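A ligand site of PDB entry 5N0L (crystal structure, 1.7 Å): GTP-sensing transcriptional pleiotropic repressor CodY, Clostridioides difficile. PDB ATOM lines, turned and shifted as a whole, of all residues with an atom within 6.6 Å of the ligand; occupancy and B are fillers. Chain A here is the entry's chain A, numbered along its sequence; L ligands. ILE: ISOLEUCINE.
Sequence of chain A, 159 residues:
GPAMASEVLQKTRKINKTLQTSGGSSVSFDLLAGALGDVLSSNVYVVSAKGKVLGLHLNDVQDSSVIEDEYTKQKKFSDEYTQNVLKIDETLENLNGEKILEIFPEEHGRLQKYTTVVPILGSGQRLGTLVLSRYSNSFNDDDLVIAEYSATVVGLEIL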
ATOM      1  N   ASN A  43      12.058   8.125 -20.871  1.00  0.00           N
ATOM      2  CA  ASN A  43      12.693   9.544 -20.852  1.00  0.00           C
ATOM      3  C   ASN A  43      13.963   9.443 -20.069  1.00  0.00           C
ATOM      4  O   ASN A  43      13.950   8.908 -18.985  1.00  0.00           O
ATOM      5  CB  ASN A  43      11.719  10.487 -20.145  1.00  0.00           C
ATOM      6  CG  ASN A  43      10.524  10.898 -21.021  1.00  0.00           C
ATOM      7  OD1 ASN A  43      10.421  10.494 -22.209  1.00  0.00           O
ATOM      8  ND2 ASN A  43       9.629  11.780 -20.450  1.00  0.00           N
ATOM      9  N   VAL A  44      15.053   9.995 -20.590  1.00  0.00           N
ATOM     10  CA  VAL A  44      16.341  10.006 -19.987  1.00  0.00           C
ATOM     11  C   VAL A  44      16.855  11.492 -19.914  1.00  0.00           C
ATOM     12  O   VAL A  44      16.914  12.151 -20.976  1.00  0.00           O
ATOM     13  CB  VAL A  44      17.304   9.262 -20.870  1.00  0.00           C
ATOM     14  CG1 VAL A  44      18.674   9.133 -20.343  1.00  0.00           C
ATOM     15  CG2 VAL A  44      16.697   7.797 -21.127  1.00  0.00           C
ATOM     16  N   TYR A  45      17.242  11.839 -18.740  1.00  0.00           N
ATOM     17  CA  TYR A  45      17.921  13.149 -18.494  1.00  0.00           C
ATOM     18  C   TYR A  45      19.267  12.970 -17.882  1.00  0.00           C
ATOM     19  O   TYR A  45      19.407  12.287 -16.826  1.00  0.00           O
ATOM     20  CB  TYR A  45      17.044  13.929 -17.592  1.00  0.00           C
ATOM     21  CG  TYR A  45      15.611  14.073 -17.904  1.00  0.00           C
ATOM     22  CD1 TYR A  45      14.638  13.092 -17.489  1.00  0.00           C
ATOM     23  CD2 TYR A  45      15.080  15.173 -18.549  1.00  0.00           C
ATOM     24  CE1 TYR A  45      13.345  13.202 -17.698  1.00  0.00           C
ATOM     25  CE2 TYR A  45      13.741  15.316 -18.774  1.00  0.00           C
ATOM     26  CZ  TYR A  45      12.824  14.382 -18.352  1.00  0.00           C
ATOM     27  OH  TYR A  45      11.471  14.489 -18.557  1.00  0.00           O
ATOM     28  N   LEU A  58      13.545  11.849 -25.113  1.00  0.00           N
ATOM     29  CA  LEU A  58      12.095  11.844 -24.683  1.00  0.00           C
ATOM     30  C   LEU A  58      11.292  10.790 -25.410  1.00  0.00           C
ATOM     31  O   LEU A  58      10.964  10.934 -26.573  1.00  0.00           O
ATOM     32  CB  LEU A  58      11.424  13.259 -24.877  1.00  0.00           C
ATOM     33  CG  LEU A  58      12.025  14.360 -24.006  1.00  0.00           C
ATOM     34  CD1 LEU A  58      11.409  15.721 -24.499  1.00  0.00           C
ATOM     35  CD2 LEU A  58      11.829  14.132 -22.478  1.00  0.00           C
ATOM     36  N   ASP A  60       8.322  10.077 -24.092  1.00  0.00           N
ATOM     37  CA  ASP A  60       7.038  10.644 -23.829  1.00  0.00           C
ATOM     38  C   ASP A  60       7.238  12.207 -23.756  1.00  0.00           C
ATOM     39  O   ASP A  60       7.532  12.728 -22.728  1.00  0.00           O
ATOM     40  CB  ASP A  60       6.469  10.142 -22.558  1.00  0.00           C
ATOM     41  CG  ASP A  60       6.327   8.558 -22.609  1.00  0.00           C
ATOM     42  OD1 ASP A  60       5.325   8.157 -23.193  1.00  0.00           O
ATOM     43  OD2 ASP A  60       7.292   7.852 -22.188  1.00  0.00           O
ATOM     44  N   ASP A  63       5.741  14.788 -21.106  1.00  0.00           N
ATOM     45  CA  ASP A  63       6.177  14.741 -19.735  1.00  0.00           C
ATOM     46  C   ASP A  63       7.528  15.340 -19.420  1.00  0.00           C
ATOM     47  O   ASP A  63       7.991  15.235 -18.294  1.00  0.00           O
ATOM     48  CB  ASP A  63       6.257  13.139 -19.344  1.00  0.00           C
ATOM     49  CG  ASP A  63       4.942  12.448 -19.456  1.00  0.00           C
ATOM     50  OD1 ASP A  63       3.895  13.095 -19.675  1.00  0.00           O
ATOM     51  OD2 ASP A  63       4.965  11.165 -19.234  1.00  0.00           O
ATOM     52  N   SER A  64       8.137  16.104 -20.382  1.00  0.00           N
ATOM     53  CA  SER A  64       9.461  16.667 -20.149  1.00  0.00           C
ATOM     54  C   SER A  64       9.449  17.632 -18.998  1.00  0.00           C
ATOM     55  O   SER A  64       8.520  18.437 -18.920  1.00  0.00           O
ATOM     56  CB  SER A  64       9.964  17.373 -21.370  1.00  0.00           C
ATOM     57  OG  SER A  64      11.215  17.886 -21.030  1.00  0.00           O
ATOM     58  N   SER A  65      10.410  17.545 -18.130  1.00  0.00           N
ATOM     59  CA  SER A  65      10.581  18.537 -17.046  1.00  0.00           C
ATOM     60  C   SER A  65      11.657  19.604 -17.393  1.00  0.00           C
ATOM     61  O   SER A  65      12.099  20.301 -16.516  1.00  0.00           O
ATOM     62  CB  SER A  65      10.962  17.867 -15.718  1.00  0.00           C
ATOM     63  OG  SER A  65       9.819  17.215 -15.213  1.00  0.00           O
ATOM     64  N   VAL A  66      12.141  19.560 -18.611  1.00  0.00           N
ATOM     65  CA  VAL A  66      13.188  20.502 -19.072  1.00  0.00           C
ATOM     66  C   VAL A  66      12.521  21.851 -19.191  1.00  0.00           C
ATOM     67  O   VAL A  66      11.390  22.017 -19.616  1.00  0.00           O
ATOM     68  CB  VAL A  66      13.790  20.134 -20.429  1.00  0.00           C
ATOM     69  CG1 VAL A  66      14.855  21.113 -20.808  1.00  0.00           C
ATOM     70  CG2 VAL A  66      14.554  18.778 -20.427  1.00  0.00           C
ATOM     71  N   PHE A  77      16.964  21.762 -15.324  1.00  0.00           N
ATOM     72  CA  PHE A  77      15.904  21.511 -14.328  1.00  0.00           C
ATOM     73  C   PHE A  77      15.657  22.774 -13.486  1.00  0.00           C
ATOM     74  O   PHE A  77      16.572  23.624 -13.284  1.00  0.00           O
ATOM     75  CB  PHE A  77      16.203  20.333 -13.375  1.00  0.00           C
ATOM     76  CG  PHE A  77      15.859  18.952 -13.942  1.00  0.00           C
ATOM     77  CD1 PHE A  77      15.370  18.710 -15.205  1.00  0.00           C
ATOM     78  CD2 PHE A  77      16.190  17.907 -13.113  1.00  0.00           C
ATOM     79  CE1 PHE A  77      15.085  17.369 -15.662  1.00  0.00           C
ATOM     80  CE2 PHE A  77      15.888  16.599 -13.566  1.00  0.00           C
ATOM     81  CZ  PHE A  77      15.400  16.351 -14.807  1.00  0.00           C
ATOM     82  N   TYR A  81      13.959  20.958  -8.497  1.00  0.00           N
ATOM     83  CA  TYR A  81      14.366  19.602  -8.988  1.00  0.00           C
ATOM     84  C   TYR A  81      15.858  19.414  -8.885  1.00  0.00           C
ATOM     85  O   TYR A  81      16.334  18.344  -8.500  1.00  0.00           O
ATOM     86  CB  TYR A  81      13.893  19.361 -10.416  1.00  0.00           C
ATOM     87  CG  TYR A  81      12.407  19.032 -10.610  1.00  0.00           C
ATOM     88  CD1 TYR A  81      11.419  19.396  -9.692  1.00  0.00           C
ATOM     89  CD2 TYR A  81      11.983  18.282 -11.712  1.00  0.00           C
ATOM     90  CE1 TYR A  81      10.082  19.049  -9.890  1.00  0.00           C
ATOM     91  CE2 TYR A  81      10.611  17.900 -11.901  1.00  0.00           C
ATOM     92  CZ  TYR A  81       9.687  18.295 -10.993  1.00  0.00           C
ATOM     93  OH  TYR A  81       8.370  17.927 -11.095  1.00  0.00           O
ATOM     94  N   ILE A 100       6.788  10.101  -5.610  1.00  0.00           N
ATOM     95  CA  ILE A 100       7.495  10.859  -6.638  1.00  0.00           C
ATOM     96  C   ILE A 100       7.552  12.316  -6.195  1.00  0.00           C
ATOM     97  O   ILE A 100       8.574  12.979  -6.399  1.00  0.00           O
ATOM     98  CB  ILE A 100       6.787  10.743  -7.999  1.00  0.00           C
ATOM     99  CG1 ILE A 100       7.035   9.364  -8.671  1.00  0.00           C
ATOM    100  CG2 ILE A 100       7.350  11.719  -9.006  1.00  0.00           C
ATOM    101  CD1 ILE A 100       5.960   9.048  -9.691  1.00  0.00           C
ATOM    102  N   PHE A 104      10.150  15.303  -6.868  1.00  0.00           N
ATOM    103  CA  PHE A 104       9.766  16.005  -8.100  1.00  0.00           C
ATOM    104  C   PHE A 104       8.376  16.535  -7.874  1.00  0.00           C
ATOM    105  O   PHE A 104       7.360  15.897  -8.281  1.00  0.00           O
ATOM    106  CB  PHE A 104       9.842  15.080  -9.314  1.00  0.00           C
ATOM    107  CG  PHE A 104      11.156  14.503  -9.557  1.00  0.00           C
ATOM    108  CD1 PHE A 104      12.274  15.258  -9.940  1.00  0.00           C
ATOM    109  CD2 PHE A 104      11.340  13.088  -9.469  1.00  0.00           C
ATOM    110  CE1 PHE A 104      13.479  14.700 -10.201  1.00  0.00           C
ATOM    111  CE2 PHE A 104      12.564  12.505  -9.694  1.00  0.00           C
ATOM    112  CZ  PHE A 104      13.663  13.273 -10.079  1.00  0.00           C
ATOM    113  N   GLU A 106       6.269  18.662  -9.101  1.00  0.00           N
ATOM    114  CA  GLU A 106       5.371  19.065 -10.135  1.00  0.00           C
ATOM    115  C   GLU A 106       4.867  17.921 -10.972  1.00  0.00           C
ATOM    116  O   GLU A 106       4.431  18.097 -12.136  1.00  0.00           O
ATOM    117  CB  GLU A 106       6.108  20.061 -11.105  1.00  0.00           C
ATOM    118  CG  GLU A 106       6.716  21.275 -10.454  1.00  0.00           C
ATOM    119  CD  GLU A 106       5.723  21.933  -9.560  1.00  0.00           C
ATOM    120  OE1 GLU A 106       4.632  22.289 -10.081  1.00  0.00           O
ATOM    121  OE2 GLU A 106       5.992  22.036  -8.336  1.00  0.00           O
ATOM    122  N   GLU A 107       4.889  16.723 -10.420  1.00  0.00           N
ATOM    123  CA  GLU A 107       4.552  15.624 -11.245  1.00  0.00           C
ATOM    124  C   GLU A 107       3.108  15.167 -11.166  1.00  0.00           C
ATOM    125  O   GLU A 107       2.821  13.962 -11.571  1.00  0.00           O
ATOM    126  CB  GLU A 107       5.484  14.424 -10.928  1.00  0.00           C
ATOM    127  CG  GLU A 107       6.914  14.672 -11.298  1.00  0.00           C
ATOM    128  CD  GLU A 107       7.101  15.063 -12.749  1.00  0.00           C
ATOM    129  OE1 GLU A 107       6.742  14.201 -13.585  1.00  0.00           O
ATOM    130  OE2 GLU A 107       7.618  16.240 -13.029  1.00  0.00           O
ATOM    131  N   ARG A 110       1.426  12.541 -13.476  1.00  0.00           N
ATOM    132  CA  ARG A 110       2.401  11.564 -14.011  1.00  0.00           C
ATOM    133  C   ARG A 110       2.824  10.618 -12.881  1.00  0.00           C
ATOM    134  O   ARG A 110       3.958  10.157 -12.842  1.00  0.00           O
ATOM    135  CB  ARG A 110       3.631  12.291 -14.599  1.00  0.00           C
ATOM    136  CG  ARG A 110       3.311  13.180 -15.794  1.00  0.00           C
ATOM    137  CD  ARG A 110       4.543  13.778 -16.446  1.00  0.00           C
ATOM    138  NE  ARG A 110       5.228  14.852 -15.697  1.00  0.00           N
ATOM    139  CZ  ARG A 110       5.215  16.155 -16.005  1.00  0.00           C
ATOM    140  NH1 ARG A 110       5.913  17.005 -15.279  1.00  0.00           N
ATOM    141  NH2 ARG A 110       4.487  16.628 -17.014  1.00  0.00           N
ATOM    142  N   LYS A 113       4.036   6.724 -13.285  1.00  0.00           N
ATOM    143  CA  LYS A 113       5.321   6.400 -13.838  1.00  0.00           C
ATOM    144  C   LYS A 113       6.299   5.824 -12.800  1.00  0.00           C
ATOM    145  O   LYS A 113       6.096   5.944 -11.605  1.00  0.00           O
ATOM    146  CB  LYS A 113       5.954   7.693 -14.416  1.00  0.00           C
ATOM    147  CG  LYS A 113       5.083   8.180 -15.563  1.00  0.00           C
ATOM    148  CD  LYS A 113       5.691   9.383 -16.274  1.00  0.00           C
ATOM    149  CE  LYS A 113       6.754   8.975 -17.217  1.00  0.00           C
ATOM    150  NZ  LYS A 113       7.325  10.076 -18.077  1.00  0.00           N
ATOM    151  N   THR A 115      10.203   5.986 -11.903  1.00  0.00           N
ATOM    152  CA  THR A 115      11.396   6.816 -12.102  1.00  0.00           C
ATOM    153  C   THR A 115      12.589   6.313 -11.267  1.00  0.00           C
ATOM    154  O   THR A 115      12.448   6.027 -10.057  1.00  0.00           O
ATOM    155  CB  THR A 115      11.030   8.286 -11.721  1.00  0.00           C
ATOM    156  OG1 THR A 115       9.976   8.700 -12.605  1.00  0.00           O
ATOM    157  CG2 THR A 115      12.350   9.166 -11.907  1.00  0.00           C
ATOM    158  N   VAL A 131      18.528  10.511 -14.691  1.00  0.00           N
ATOM    159  CA  VAL A 131      17.105  10.329 -14.387  1.00  0.00           C
ATOM    160  C   VAL A 131      16.421   9.609 -15.533  1.00  0.00           C
ATOM    161  O   VAL A 131      16.583   9.905 -16.736  1.00  0.00           O
ATOM    162  CB  VAL A 131      16.377  11.672 -14.111  1.00  0.00           C
ATOM    163  CG1 VAL A 131      14.935  11.409 -13.768  1.00  0.00           C
ATOM    164  CG2 VAL A 131      17.034  12.421 -12.990  1.00  0.00           C
ATOM    165  N   LEU A 132      15.758   8.460 -15.201  1.00  0.00           N
ATOM    166  CA  LEU A 132      15.165   7.623 -16.182  1.00  0.00           C
ATOM    167  C   LEU A 132      13.740   7.398 -15.756  1.00  0.00           C
ATOM    168  O   LEU A 132      13.480   7.222 -14.574  1.00  0.00           O
ATOM    169  CB  LEU A 132      15.854   6.254 -16.276  1.00  0.00           C
ATOM    170  CG  LEU A 132      17.340   6.366 -16.578  1.00  0.00           C
ATOM    171  CD1 LEU A 132      18.091   5.656 -15.518  1.00  0.00           C
ATOM    172  CD2 LEU A 132      17.742   5.839 -17.920  1.00  0.00           C
ATOM    173  N   SER A 133      12.809   7.514 -16.705  1.00  0.00           N
ATOM    174  CA  SER A 133      11.402   7.462 -16.369  1.00  0.00           C
ATOM    175  C   SER A 133      10.535   6.875 -17.432  1.00  0.00           C
ATOM    176  O   SER A 133      10.752   7.111 -18.594  1.00  0.00           O
ATOM    177  CB  SER A 133      10.912   8.823 -15.987  1.00  0.00           C
ATOM    178  OG  SER A 133       9.570   8.868 -15.554  1.00  0.00           O
ATOM    179  N   ARG A 134       9.572   5.986 -17.059  1.00  0.00           N
ATOM    180  CA  ARG A 134       8.741   5.341 -18.039  1.00  0.00           C
ATOM    181  C   ARG A 134       7.422   4.864 -17.399  1.00  0.00           C
ATOM    182  O   ARG A 134       7.274   4.761 -16.157  1.00  0.00           O
ATOM    183  CB  ARG A 134       9.479   4.197 -18.750  1.00  0.00           C
ATOM    184  CG  ARG A 134       9.655   2.998 -17.765  1.00  0.00           C
ATOM    185  CD  ARG A 134      10.525   2.011 -18.446  1.00  0.00           C
ATOM    186  NE  ARG A 134      10.695   0.727 -17.658  1.00  0.00           N
ATOM    187  CZ  ARG A 134      11.605  -0.176 -17.949  1.00  0.00           C
ATOM    188  NH1 ARG A 134      12.436  -0.061 -18.974  1.00  0.00           N
ATOM    189  NH2 ARG A 134      11.635  -1.360 -17.196  1.00  0.00           N
ATOM    190  N   TYR A 135       6.463   4.629 -18.227  1.00  0.00           N
ATOM    191  CA  TYR A 135       5.147   4.149 -17.822  1.00  0.00           C
ATOM    192  C   TYR A 135       5.252   2.579 -17.777  1.00  0.00           C
ATOM    193  O   TYR A 135       6.142   1.995 -18.354  1.00  0.00           O
ATOM    194  CB  TYR A 135       4.056   4.448 -18.823  1.00  0.00           C
ATOM    195  CG  TYR A 135       3.701   6.021 -18.845  1.00  0.00           C
ATOM    196  CD1 TYR A 135       2.859   6.503 -17.920  1.00  0.00           C
ATOM    197  CD2 TYR A 135       4.288   6.835 -19.734  1.00  0.00           C
ATOM    198  CE1 TYR A 135       2.530   7.846 -17.810  1.00  0.00           C
ATOM    199  CE2 TYR A 135       3.958   8.189 -19.709  1.00  0.00           C
ATOM    200  CZ  TYR A 135       3.128   8.683 -18.726  1.00  0.00           C
ATOM    201  OH  TYR A 135       2.811  10.045 -18.662  1.00  0.00           O
HETATM  202  N   ILE L   1       8.670  14.813 -15.684  1.00  0.00           N
HETATM  203  CA  ILE L   1       9.741  13.777 -15.800  1.00  0.00           C
HETATM  204  C   ILE L   1       9.313  12.722 -16.794  1.00  0.00           C
HETATM  205  O   ILE L   1       8.207  12.208 -16.660  1.00  0.00           O
HETATM  206  CB  ILE L   1      10.040  13.175 -14.442  1.00  0.00           C
HETATM  207  CG1 ILE L   1      10.651  14.269 -13.549  1.00  0.00           C
HETATM  208  CG2 ILE L   1      11.068  12.115 -14.551  1.00  0.00           C
HETATM  209  CD1 ILE L   1      12.102  14.590 -13.814  1.00  0.00           C
HETATM  210  OXT ILE L   1      10.046  12.507 -17.731  1.00  0.00           O
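The side-chain hydroxyl of Tyr 45 sits at hydrogen-bond distance from an oxygen (OXT) of the ligand.
The side-chain hydroxyl of Ser 65 is in hydrogen-bond range of a nitrogen (N) of the ligand.
NZ of Lys 113 lies within salt-bridge range of O of the ligand, at 2.7 Å.
The backbone carbonyl oxygen (O) of Asp 63 lies within hydrogen-bond range of a nitrogen (N) of the ligand (2.7 Å).
ND2 of Asn 43 sits at hydrogen-bond distance from OXT of the ligand.
OE1 of Glu 107 is in salt-bridge range of N of the ligand (2.9 Å).
A nitrogen (N) of the ligand lies close to the guanidinium group (NE) of Arg 110.
The backbone carbonyl oxygen (O) of Val 131 is in hydrogen-bond range of the backbone NH (N) of Tyr 45, at 2.9 Å.
The side-chain carboxylate (OD2) of Asp 63 lies within salt-bridge range of the side-chain amino group (NZ) of Lys 113 (2.8 Å).
OD2 of Asp 63 lies within hydrogen-bond range of OH of Tyr 135 (2.5 Å).
OD1 of Asn 43 is in hydrogen-bond range of N of Asp 60 (2.9 Å).
NE of Arg 110 is in salt-bridge range of OE1 of Glu 107 (2.7 Å).
The side-chain hydroxyl (OH) of Tyr 81 sits at hydrogen-bond distance from the side-chain carboxylate (OE2) of Glu 107 (2.7 Å).
OG of Ser 133 is in hydrogen-bond range of OG1 of Thr 115 (3.0 Å).
The backbone NH of Glu 106 sits at hydrogen-bond distance from the side-chain hydroxyl of Tyr 81 (3.0 Å).
Phe 77 touches the ligand.
Tyr 81 touches the ligand.
Phe 104 touches the ligand (CE1 to CD1, 3.9 Å).
Ser 133 touches the ligand (CB to CG2, 3.6 Å).
Hydrophobic or aromatic side chains that line the ligand: Tyr 45, Phe 77, Tyr 81 and Phe 104.
Within 4 Å of the ligand: Asn 43, Tyr 45, Asp 63, Ser 65, Phe 77, Tyr 81, Phe 104, Glu 107, Arg 110, Lys 113 and Ser 133.
The nearest printed residue that does not touch the ligand is Val 131 (4.01 Å).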
